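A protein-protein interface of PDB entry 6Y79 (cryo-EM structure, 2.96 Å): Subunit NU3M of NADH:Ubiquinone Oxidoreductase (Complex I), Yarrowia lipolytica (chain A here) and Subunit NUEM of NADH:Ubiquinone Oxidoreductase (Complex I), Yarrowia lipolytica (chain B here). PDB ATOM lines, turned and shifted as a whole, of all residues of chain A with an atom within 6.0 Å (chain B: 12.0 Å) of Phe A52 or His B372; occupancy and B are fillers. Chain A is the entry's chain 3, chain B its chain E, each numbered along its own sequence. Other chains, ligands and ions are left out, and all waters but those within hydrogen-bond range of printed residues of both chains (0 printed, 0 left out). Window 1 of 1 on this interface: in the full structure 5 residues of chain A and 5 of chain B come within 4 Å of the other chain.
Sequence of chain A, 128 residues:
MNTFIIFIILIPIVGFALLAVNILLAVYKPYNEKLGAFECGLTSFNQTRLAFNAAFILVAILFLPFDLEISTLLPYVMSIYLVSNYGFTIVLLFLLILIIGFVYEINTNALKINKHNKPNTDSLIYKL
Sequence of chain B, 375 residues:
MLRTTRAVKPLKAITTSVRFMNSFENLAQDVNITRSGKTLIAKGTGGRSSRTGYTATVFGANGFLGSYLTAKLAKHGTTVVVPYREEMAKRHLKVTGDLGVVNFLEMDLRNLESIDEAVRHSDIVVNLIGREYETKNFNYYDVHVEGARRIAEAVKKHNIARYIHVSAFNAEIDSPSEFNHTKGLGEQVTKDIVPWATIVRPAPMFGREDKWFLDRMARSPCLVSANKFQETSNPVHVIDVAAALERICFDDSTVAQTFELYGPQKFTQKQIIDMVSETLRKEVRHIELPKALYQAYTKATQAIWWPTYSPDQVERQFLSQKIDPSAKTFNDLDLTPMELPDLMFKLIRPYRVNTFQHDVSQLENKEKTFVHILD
Of the 7 printed residues of chain A, 4 touch a printed residue of chain B.
Hydrophobic or aromatic side chains of chain A that line the printed part of chain B: Ala A51 and Phe A52.
Among the printed residues, 9 pairs touch across the chains.
Among the printed residues, no Asp or Glu carboxylate lies within 4 Å of a Lys or Arg side-chain nitrogen of the other chain.
Of the printed residues of chain B, Phe A52 touches His B372, Ile B373 and Leu B374.
His B372 touches just these residues of chain A: Ala A51 (3.3 Å) and Phe A52 (3.8 Å).
No residue of chain B comes within 4 Å of Leu A50.
Of chain B, only Val B371, His B372 and Leu B374 come within 4 Å of Ala A51.
Phe A56 touches none of the printed residues of chain B.
No residue of chain B comes within 4 Å of Ile A57.
Printed residues of chain A within 4 Å of Ile B373: Phe A52 (2.8 Å), Asn A53 (3.9 Å) and Ala A54 (3.97 Å).
Printed residues of chain A within 4 Å of Val B371: Ala A51.
Of the printed residues of chain A, Leu B374 touches Ala A51, Phe A52 and Asn A53.
Glu B364 touches none of the printed residues of chain A.
The nearest printed residue of chain B that does not touch Phe A52 is Val B371 (6.7 Å).
The nearest residue of chain A that does not touch His B372 is Leu A50 (4.8 Å).
O of Phe A52 sits close to O of Ile B373 (2.8 Å).
Among the printed residues, pairs that only touch across the chains: Ala A51 with Val B371 (3.8 Å), Ala A51 with His B372 (3.3 Å), Ala A51 with Leu B374 (3.7 Å), Phe A52 with His B372 (3.8 Å), Phe A52 with Leu B374 (3.99 Å), Asn A53 with Ile B373 (3.9 Å), Asn A53 with Leu B374 (3.6 Å) and Ala A54 with Ile B373 (3.97 Å).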
ATOM      1  N   LEU A  50     -18.714 -23.398 -24.801  1.00  0.00           N
ATOM      2  CA  LEU A  50     -18.870 -24.772 -24.356  1.00  0.00           C
ATOM      3  C   LEU A  50     -17.779 -25.125 -23.360  1.00  0.00           C
ATOM      4  O   LEU A  50     -16.758 -24.443 -23.256  1.00  0.00           O
ATOM      5  CB  LEU A  50     -18.860 -25.759 -25.537  1.00  0.00           C
ATOM      6  CG  LEU A  50     -17.700 -25.869 -26.533  1.00  0.00           C
ATOM      7  CD1 LEU A  50     -16.605 -26.858 -26.120  1.00  0.00           C
ATOM      8  CD2 LEU A  50     -18.250 -26.227 -27.899  1.00  0.00           C
ATOM      9  N   ALA A  51     -18.020 -26.198 -22.622  1.00  0.00           N
ATOM     10  CA  ALA A  51     -17.033 -26.762 -21.726  1.00  0.00           C
ATOM     11  C   ALA A  51     -16.330 -27.931 -22.398  1.00  0.00           C
ATOM     12  O   ALA A  51     -16.882 -28.598 -23.273  1.00  0.00           O
ATOM     13  CB  ALA A  51     -17.692 -27.212 -20.427  1.00  0.00           C
ATOM     14  N   PHE A  52     -15.103 -28.177 -21.958  1.00  0.00           N
ATOM     15  CA  PHE A  52     -14.169 -29.090 -22.592  1.00  0.00           C
ATOM     16  C   PHE A  52     -13.522 -29.928 -21.505  1.00  0.00           C
ATOM     17  O   PHE A  52     -13.475 -29.521 -20.348  1.00  0.00           O
ATOM     18  CB  PHE A  52     -13.097 -28.324 -23.385  1.00  0.00           C
ATOM     19  CG  PHE A  52     -12.433 -27.230 -22.599  1.00  0.00           C
ATOM     20  CD1 PHE A  52     -12.964 -25.948 -22.573  1.00  0.00           C
ATOM     21  CD2 PHE A  52     -11.271 -27.482 -21.882  1.00  0.00           C
ATOM     22  CE1 PHE A  52     -12.366 -24.958 -21.836  1.00  0.00           C
ATOM     23  CE2 PHE A  52     -10.671 -26.487 -21.150  1.00  0.00           C
ATOM     24  CZ  PHE A  52     -11.211 -25.221 -21.140  1.00  0.00           C
ATOM     25  N   ASN A  53     -13.005 -31.093 -21.879  1.00  0.00           N
ATOM     26  CA  ASN A  53     -12.373 -31.927 -20.872  1.00  0.00           C
ATOM     27  C   ASN A  53     -10.942 -31.464 -20.616  1.00  0.00           C
ATOM     28  O   ASN A  53     -10.381 -30.653 -21.353  1.00  0.00           O
ATOM     29  CB  ASN A  53     -12.407 -33.398 -21.284  1.00  0.00           C
ATOM     30  CG  ASN A  53     -13.802 -33.862 -21.641  1.00  0.00           C
ATOM     31  OD1 ASN A  53     -14.097 -34.151 -22.796  1.00  0.00           O
ATOM     32  ND2 ASN A  53     -14.675 -33.926 -20.645  1.00  0.00           N
ATOM     33  N   ALA A  54     -10.360 -31.981 -19.533  1.00  0.00           N
ATOM     34  CA  ALA A  54      -9.070 -31.475 -19.075  1.00  0.00           C
ATOM     35  C   ALA A  54      -7.929 -31.957 -19.960  1.00  0.00           C
ATOM     36  O   ALA A  54      -6.876 -31.312 -20.031  1.00  0.00           O
ATOM     37  CB  ALA A  54      -8.831 -31.892 -17.627  1.00  0.00           C
ATOM     38  N   PHE A  56      -7.764 -32.069 -23.168  1.00  0.00           N
ATOM     39  CA  PHE A  56      -7.586 -31.183 -24.319  1.00  0.00           C
ATOM     40  C   PHE A  56      -6.592 -30.089 -24.032  1.00  0.00           C
ATOM     41  O   PHE A  56      -5.749 -29.753 -24.866  1.00  0.00           O
ATOM     42  CB  PHE A  56      -8.883 -30.490 -24.686  1.00  0.00           C
ATOM     43  CG  PHE A  56      -9.915 -31.382 -25.142  1.00  0.00           C
ATOM     44  CD1 PHE A  56      -9.918 -31.821 -26.438  1.00  0.00           C
ATOM     45  CD2 PHE A  56     -10.892 -31.786 -24.282  1.00  0.00           C
ATOM     46  CE1 PHE A  56     -10.892 -32.657 -26.882  1.00  0.00           C
ATOM     47  CE2 PHE A  56     -11.879 -32.619 -24.702  1.00  0.00           C
ATOM     48  CZ  PHE A  56     -11.859 -33.031 -25.994  1.00  0.00           C
ATOM     49  N   ILE A  57      -6.761 -29.435 -22.896  1.00  0.00           N
ATOM     50  CA  ILE A  57      -5.858 -28.355 -22.578  1.00  0.00           C
ATOM     51  C   ILE A  57      -4.549 -28.945 -22.096  1.00  0.00           C
ATOM     52  O   ILE A  57      -3.476 -28.370 -22.324  1.00  0.00           O
ATOM     53  CB  ILE A  57      -6.540 -27.407 -21.573  1.00  0.00           C
ATOM     54  CG1 ILE A  57      -5.796 -26.096 -21.526  1.00  0.00           C
ATOM     55  CG2 ILE A  57      -6.749 -28.032 -20.196  1.00  0.00           C
ATOM     56  CD1 ILE A  57      -6.085 -25.302 -22.732  1.00  0.00           C
ATOM     57  N   GLN B 362     -24.859  -9.928 -13.432  1.00  0.00           N
ATOM     58  CA  GLN B 362     -25.672 -11.033 -12.916  1.00  0.00           C
ATOM     59  C   GLN B 362     -25.348 -12.345 -13.626  1.00  0.00           C
ATOM     60  O   GLN B 362     -25.459 -13.421 -13.014  1.00  0.00           O
ATOM     61  CB  GLN B 362     -27.166 -10.684 -12.974  1.00  0.00           C
ATOM     62  CG  GLN B 362     -27.540  -9.708 -11.842  1.00  0.00           C
ATOM     63  CD  GLN B 362     -27.308  -8.271 -12.217  1.00  0.00           C
ATOM     64  OE1 GLN B 362     -27.203  -7.949 -13.397  1.00  0.00           O
ATOM     65  NE2 GLN B 362     -27.225  -7.394 -11.223  1.00  0.00           N
ATOM     66  N   LEU B 363     -24.855 -12.281 -14.883  1.00  0.00           N
ATOM     67  CA  LEU B 363     -24.447 -13.514 -15.545  1.00  0.00           C
ATOM     68  C   LEU B 363     -23.091 -13.997 -15.027  1.00  0.00           C
ATOM     69  O   LEU B 363     -22.802 -15.188 -15.139  1.00  0.00           O
ATOM     70  CB  LEU B 363     -24.465 -13.351 -17.073  1.00  0.00           C
ATOM     71  CG  LEU B 363     -24.488 -14.714 -17.802  1.00  0.00           C
ATOM     72  CD1 LEU B 363     -25.602 -15.628 -17.234  1.00  0.00           C
ATOM     73  CD2 LEU B 363     -24.620 -14.653 -19.334  1.00  0.00           C
ATOM     74  N   GLU B 364     -22.270 -13.124 -14.391  1.00  0.00           N
ATOM     75  CA  GLU B 364     -21.060 -13.661 -13.747  1.00  0.00           C
ATOM     76  C   GLU B 364     -21.415 -14.584 -12.585  1.00  0.00           C
ATOM     77  O   GLU B 364     -20.812 -15.653 -12.416  1.00  0.00           O
ATOM     78  CB  GLU B 364     -20.089 -12.571 -13.284  1.00  0.00           C
ATOM     79  CG  GLU B 364     -20.587 -11.492 -12.278  1.00  0.00           C
ATOM     80  CD  GLU B 364     -20.652 -11.925 -10.786  1.00  0.00           C
ATOM     81  OE1 GLU B 364     -19.993 -12.894 -10.350  1.00  0.00           O
ATOM     82  OE2 GLU B 364     -21.424 -11.274 -10.048  1.00  0.00           O
ATOM     83  N   ASN B 365     -22.435 -14.224 -11.804  1.00  0.00           N
ATOM     84  CA  ASN B 365     -22.746 -15.021 -10.621  1.00  0.00           C
ATOM     85  C   ASN B 365     -23.615 -16.229 -10.957  1.00  0.00           C
ATOM     86  O   ASN B 365     -23.625 -17.219 -10.201  1.00  0.00           O
ATOM     87  CB  ASN B 365     -23.422 -14.185  -9.536  1.00  0.00           C
ATOM     88  CG  ASN B 365     -23.328 -14.852  -8.177  1.00  0.00           C
ATOM     89  OD1 ASN B 365     -22.263 -14.840  -7.552  1.00  0.00           O
ATOM     90  ND2 ASN B 365     -24.407 -15.481  -7.737  1.00  0.00           N
ATOM     91  N   LYS B 366     -24.392 -16.157 -12.055  1.00  0.00           N
ATOM     92  CA  LYS B 366     -25.042 -17.384 -12.507  1.00  0.00           C
ATOM     93  C   LYS B 366     -24.043 -18.300 -13.200  1.00  0.00           C
ATOM     94  O   LYS B 366     -24.200 -19.531 -13.172  1.00  0.00           O
ATOM     95  CB  LYS B 366     -26.224 -17.073 -13.417  1.00  0.00           C
ATOM     96  CG  LYS B 366     -27.180 -18.293 -13.580  1.00  0.00           C
ATOM     97  CD  LYS B 366     -28.563 -17.970 -14.121  1.00  0.00           C
ATOM     98  CE  LYS B 366     -29.406 -19.241 -14.177  1.00  0.00           C
ATOM     99  NZ  LYS B 366     -29.009 -20.114 -15.317  1.00  0.00           N
ATOM    100  N   GLU B 367     -22.992 -17.710 -13.803  1.00  0.00           N
ATOM    101  CA  GLU B 367     -21.868 -18.485 -14.319  1.00  0.00           C
ATOM    102  C   GLU B 367     -21.124 -19.196 -13.202  1.00  0.00           C
ATOM    103  O   GLU B 367     -20.560 -20.278 -13.405  1.00  0.00           O
ATOM    104  CB  GLU B 367     -20.898 -17.582 -15.063  1.00  0.00           C
ATOM    105  CG  GLU B 367     -21.081 -17.457 -16.563  1.00  0.00           C
ATOM    106  CD  GLU B 367     -19.971 -16.649 -17.209  1.00  0.00           C
ATOM    107  OE1 GLU B 367     -18.986 -17.262 -17.653  1.00  0.00           O
ATOM    108  OE2 GLU B 367     -20.055 -15.401 -17.226  1.00  0.00           O
ATOM    109  N   LYS B 368     -21.105 -18.599 -12.016  1.00  0.00           N
ATOM    110  CA  LYS B 368     -20.482 -19.223 -10.852  1.00  0.00           C
ATOM    111  C   LYS B 368     -21.121 -20.536 -10.390  1.00  0.00           C
ATOM    112  O   LYS B 368     -20.592 -21.161  -9.471  1.00  0.00           O
ATOM    113  CB  LYS B 368     -20.486 -18.254  -9.671  1.00  0.00           C
ATOM    114  CG  LYS B 368     -19.161 -17.592  -9.364  1.00  0.00           C
ATOM    115  CD  LYS B 368     -19.371 -16.557  -8.260  1.00  0.00           C
ATOM    116  CE  LYS B 368     -18.063 -15.942  -7.817  1.00  0.00           C
ATOM    117  NZ  LYS B 368     -17.314 -15.357  -8.952  1.00  0.00           N
ATOM    118  N   THR B 369     -22.262 -20.954 -10.954  1.00  0.00           N
ATOM    119  CA  THR B 369     -22.858 -22.238 -10.601  1.00  0.00           C
ATOM    120  C   THR B 369     -22.773 -23.282 -11.706  1.00  0.00           C
ATOM    121  O   THR B 369     -23.100 -24.445 -11.455  1.00  0.00           O
ATOM    122  CB  THR B 369     -24.331 -22.070 -10.192  1.00  0.00           C
ATOM    123  OG1 THR B 369     -25.114 -21.663 -11.321  1.00  0.00           O
ATOM    124  CG2 THR B 369     -24.466 -21.044  -9.084  1.00  0.00           C
ATOM    125  N   PHE B 370     -22.343 -22.907 -12.906  1.00  0.00           N
ATOM    126  CA  PHE B 370     -22.170 -23.861 -13.991  1.00  0.00           C
ATOM    127  C   PHE B 370     -20.788 -24.500 -13.929  1.00  0.00           C
ATOM    128  O   PHE B 370     -19.952 -24.152 -13.097  1.00  0.00           O
ATOM    129  CB  PHE B 370     -22.381 -23.188 -15.348  1.00  0.00           C
ATOM    130  CG  PHE B 370     -23.797 -22.778 -15.601  1.00  0.00           C
ATOM    131  CD1 PHE B 370     -24.775 -23.728 -15.829  1.00  0.00           C
ATOM    132  CD2 PHE B 370     -24.147 -21.445 -15.614  1.00  0.00           C
ATOM    133  CE1 PHE B 370     -26.085 -23.352 -16.054  1.00  0.00           C
ATOM    134  CE2 PHE B 370     -25.453 -21.056 -15.831  1.00  0.00           C
ATOM    135  CZ  PHE B 370     -26.420 -22.012 -16.056  1.00  0.00           C
ATOM    136  N   VAL B 371     -20.557 -25.457 -14.826  1.00  0.00           N
ATOM    137  CA  VAL B 371     -19.316 -26.217 -14.892  1.00  0.00           C
ATOM    138  C   VAL B 371     -18.663 -25.927 -16.233  1.00  0.00           C
ATOM    139  O   VAL B 371     -19.332 -25.970 -17.269  1.00  0.00           O
ATOM    140  CB  VAL B 371     -19.575 -27.722 -14.721  1.00  0.00           C
ATOM    141  CG1 VAL B 371     -18.275 -28.505 -14.736  1.00  0.00           C
ATOM    142  CG2 VAL B 371     -20.306 -27.978 -13.434  1.00  0.00           C
ATOM    143  N   HIS B 372     -17.356 -25.652 -16.216  1.00  0.00           N
ATOM    144  CA  HIS B 372     -16.662 -25.173 -17.400  1.00  0.00           C
ATOM    145  C   HIS B 372     -15.495 -26.039 -17.866  1.00  0.00           C
ATOM    146  O   HIS B 372     -15.010 -25.822 -18.981  1.00  0.00           O
ATOM    147  CB  HIS B 372     -16.157 -23.742 -17.168  1.00  0.00           C
ATOM    148  CG  HIS B 372     -17.255 -22.738 -16.992  1.00  0.00           C
ATOM    149  ND1 HIS B 372     -17.713 -22.341 -15.755  1.00  0.00           N
ATOM    150  CD2 HIS B 372     -17.994 -22.060 -17.901  1.00  0.00           C
ATOM    151  CE1 HIS B 372     -18.689 -21.465 -15.910  1.00  0.00           C
ATOM    152  NE2 HIS B 372     -18.873 -21.271 -17.203  1.00  0.00           N
ATOM    153  N   ILE B 373     -15.002 -26.977 -17.048  1.00  0.00           N
ATOM    154  CA  ILE B 373     -13.846 -27.805 -17.388  1.00  0.00           C
ATOM    155  C   ILE B 373     -14.136 -29.298 -17.257  1.00  0.00           C
ATOM    156  O   ILE B 373     -13.276 -30.117 -17.582  1.00  0.00           O
ATOM    157  CB  ILE B 373     -12.604 -27.411 -16.539  1.00  0.00           C
ATOM    158  CG1 ILE B 373     -12.464 -25.898 -16.409  1.00  0.00           C
ATOM    159  CG2 ILE B 373     -11.229 -27.842 -17.137  1.00  0.00           C
ATOM    160  CD1 ILE B 373     -12.019 -25.156 -17.651  1.00  0.00           C
ATOM    161  N   LEU B 374     -15.340 -29.687 -16.825  1.00  0.00           N
ATOM    162  CA  LEU B 374     -15.745 -31.100 -16.595  1.00  0.00           C
ATOM    163  C   LEU B 374     -14.825 -31.825 -15.615  1.00  0.00           C
ATOM    164  O   LEU B 374     -13.924 -32.551 -16.034  1.00  0.00           O
ATOM    165  CB  LEU B 374     -15.804 -31.926 -17.897  1.00  0.00           C
ATOM    166  CG  LEU B 374     -17.044 -32.044 -18.774  1.00  0.00           C
ATOM    167  CD1 LEU B 374     -18.189 -32.677 -18.001  1.00  0.00           C
ATOM    168  CD2 LEU B 374     -17.421 -30.712 -19.351  1.00  0.00           C
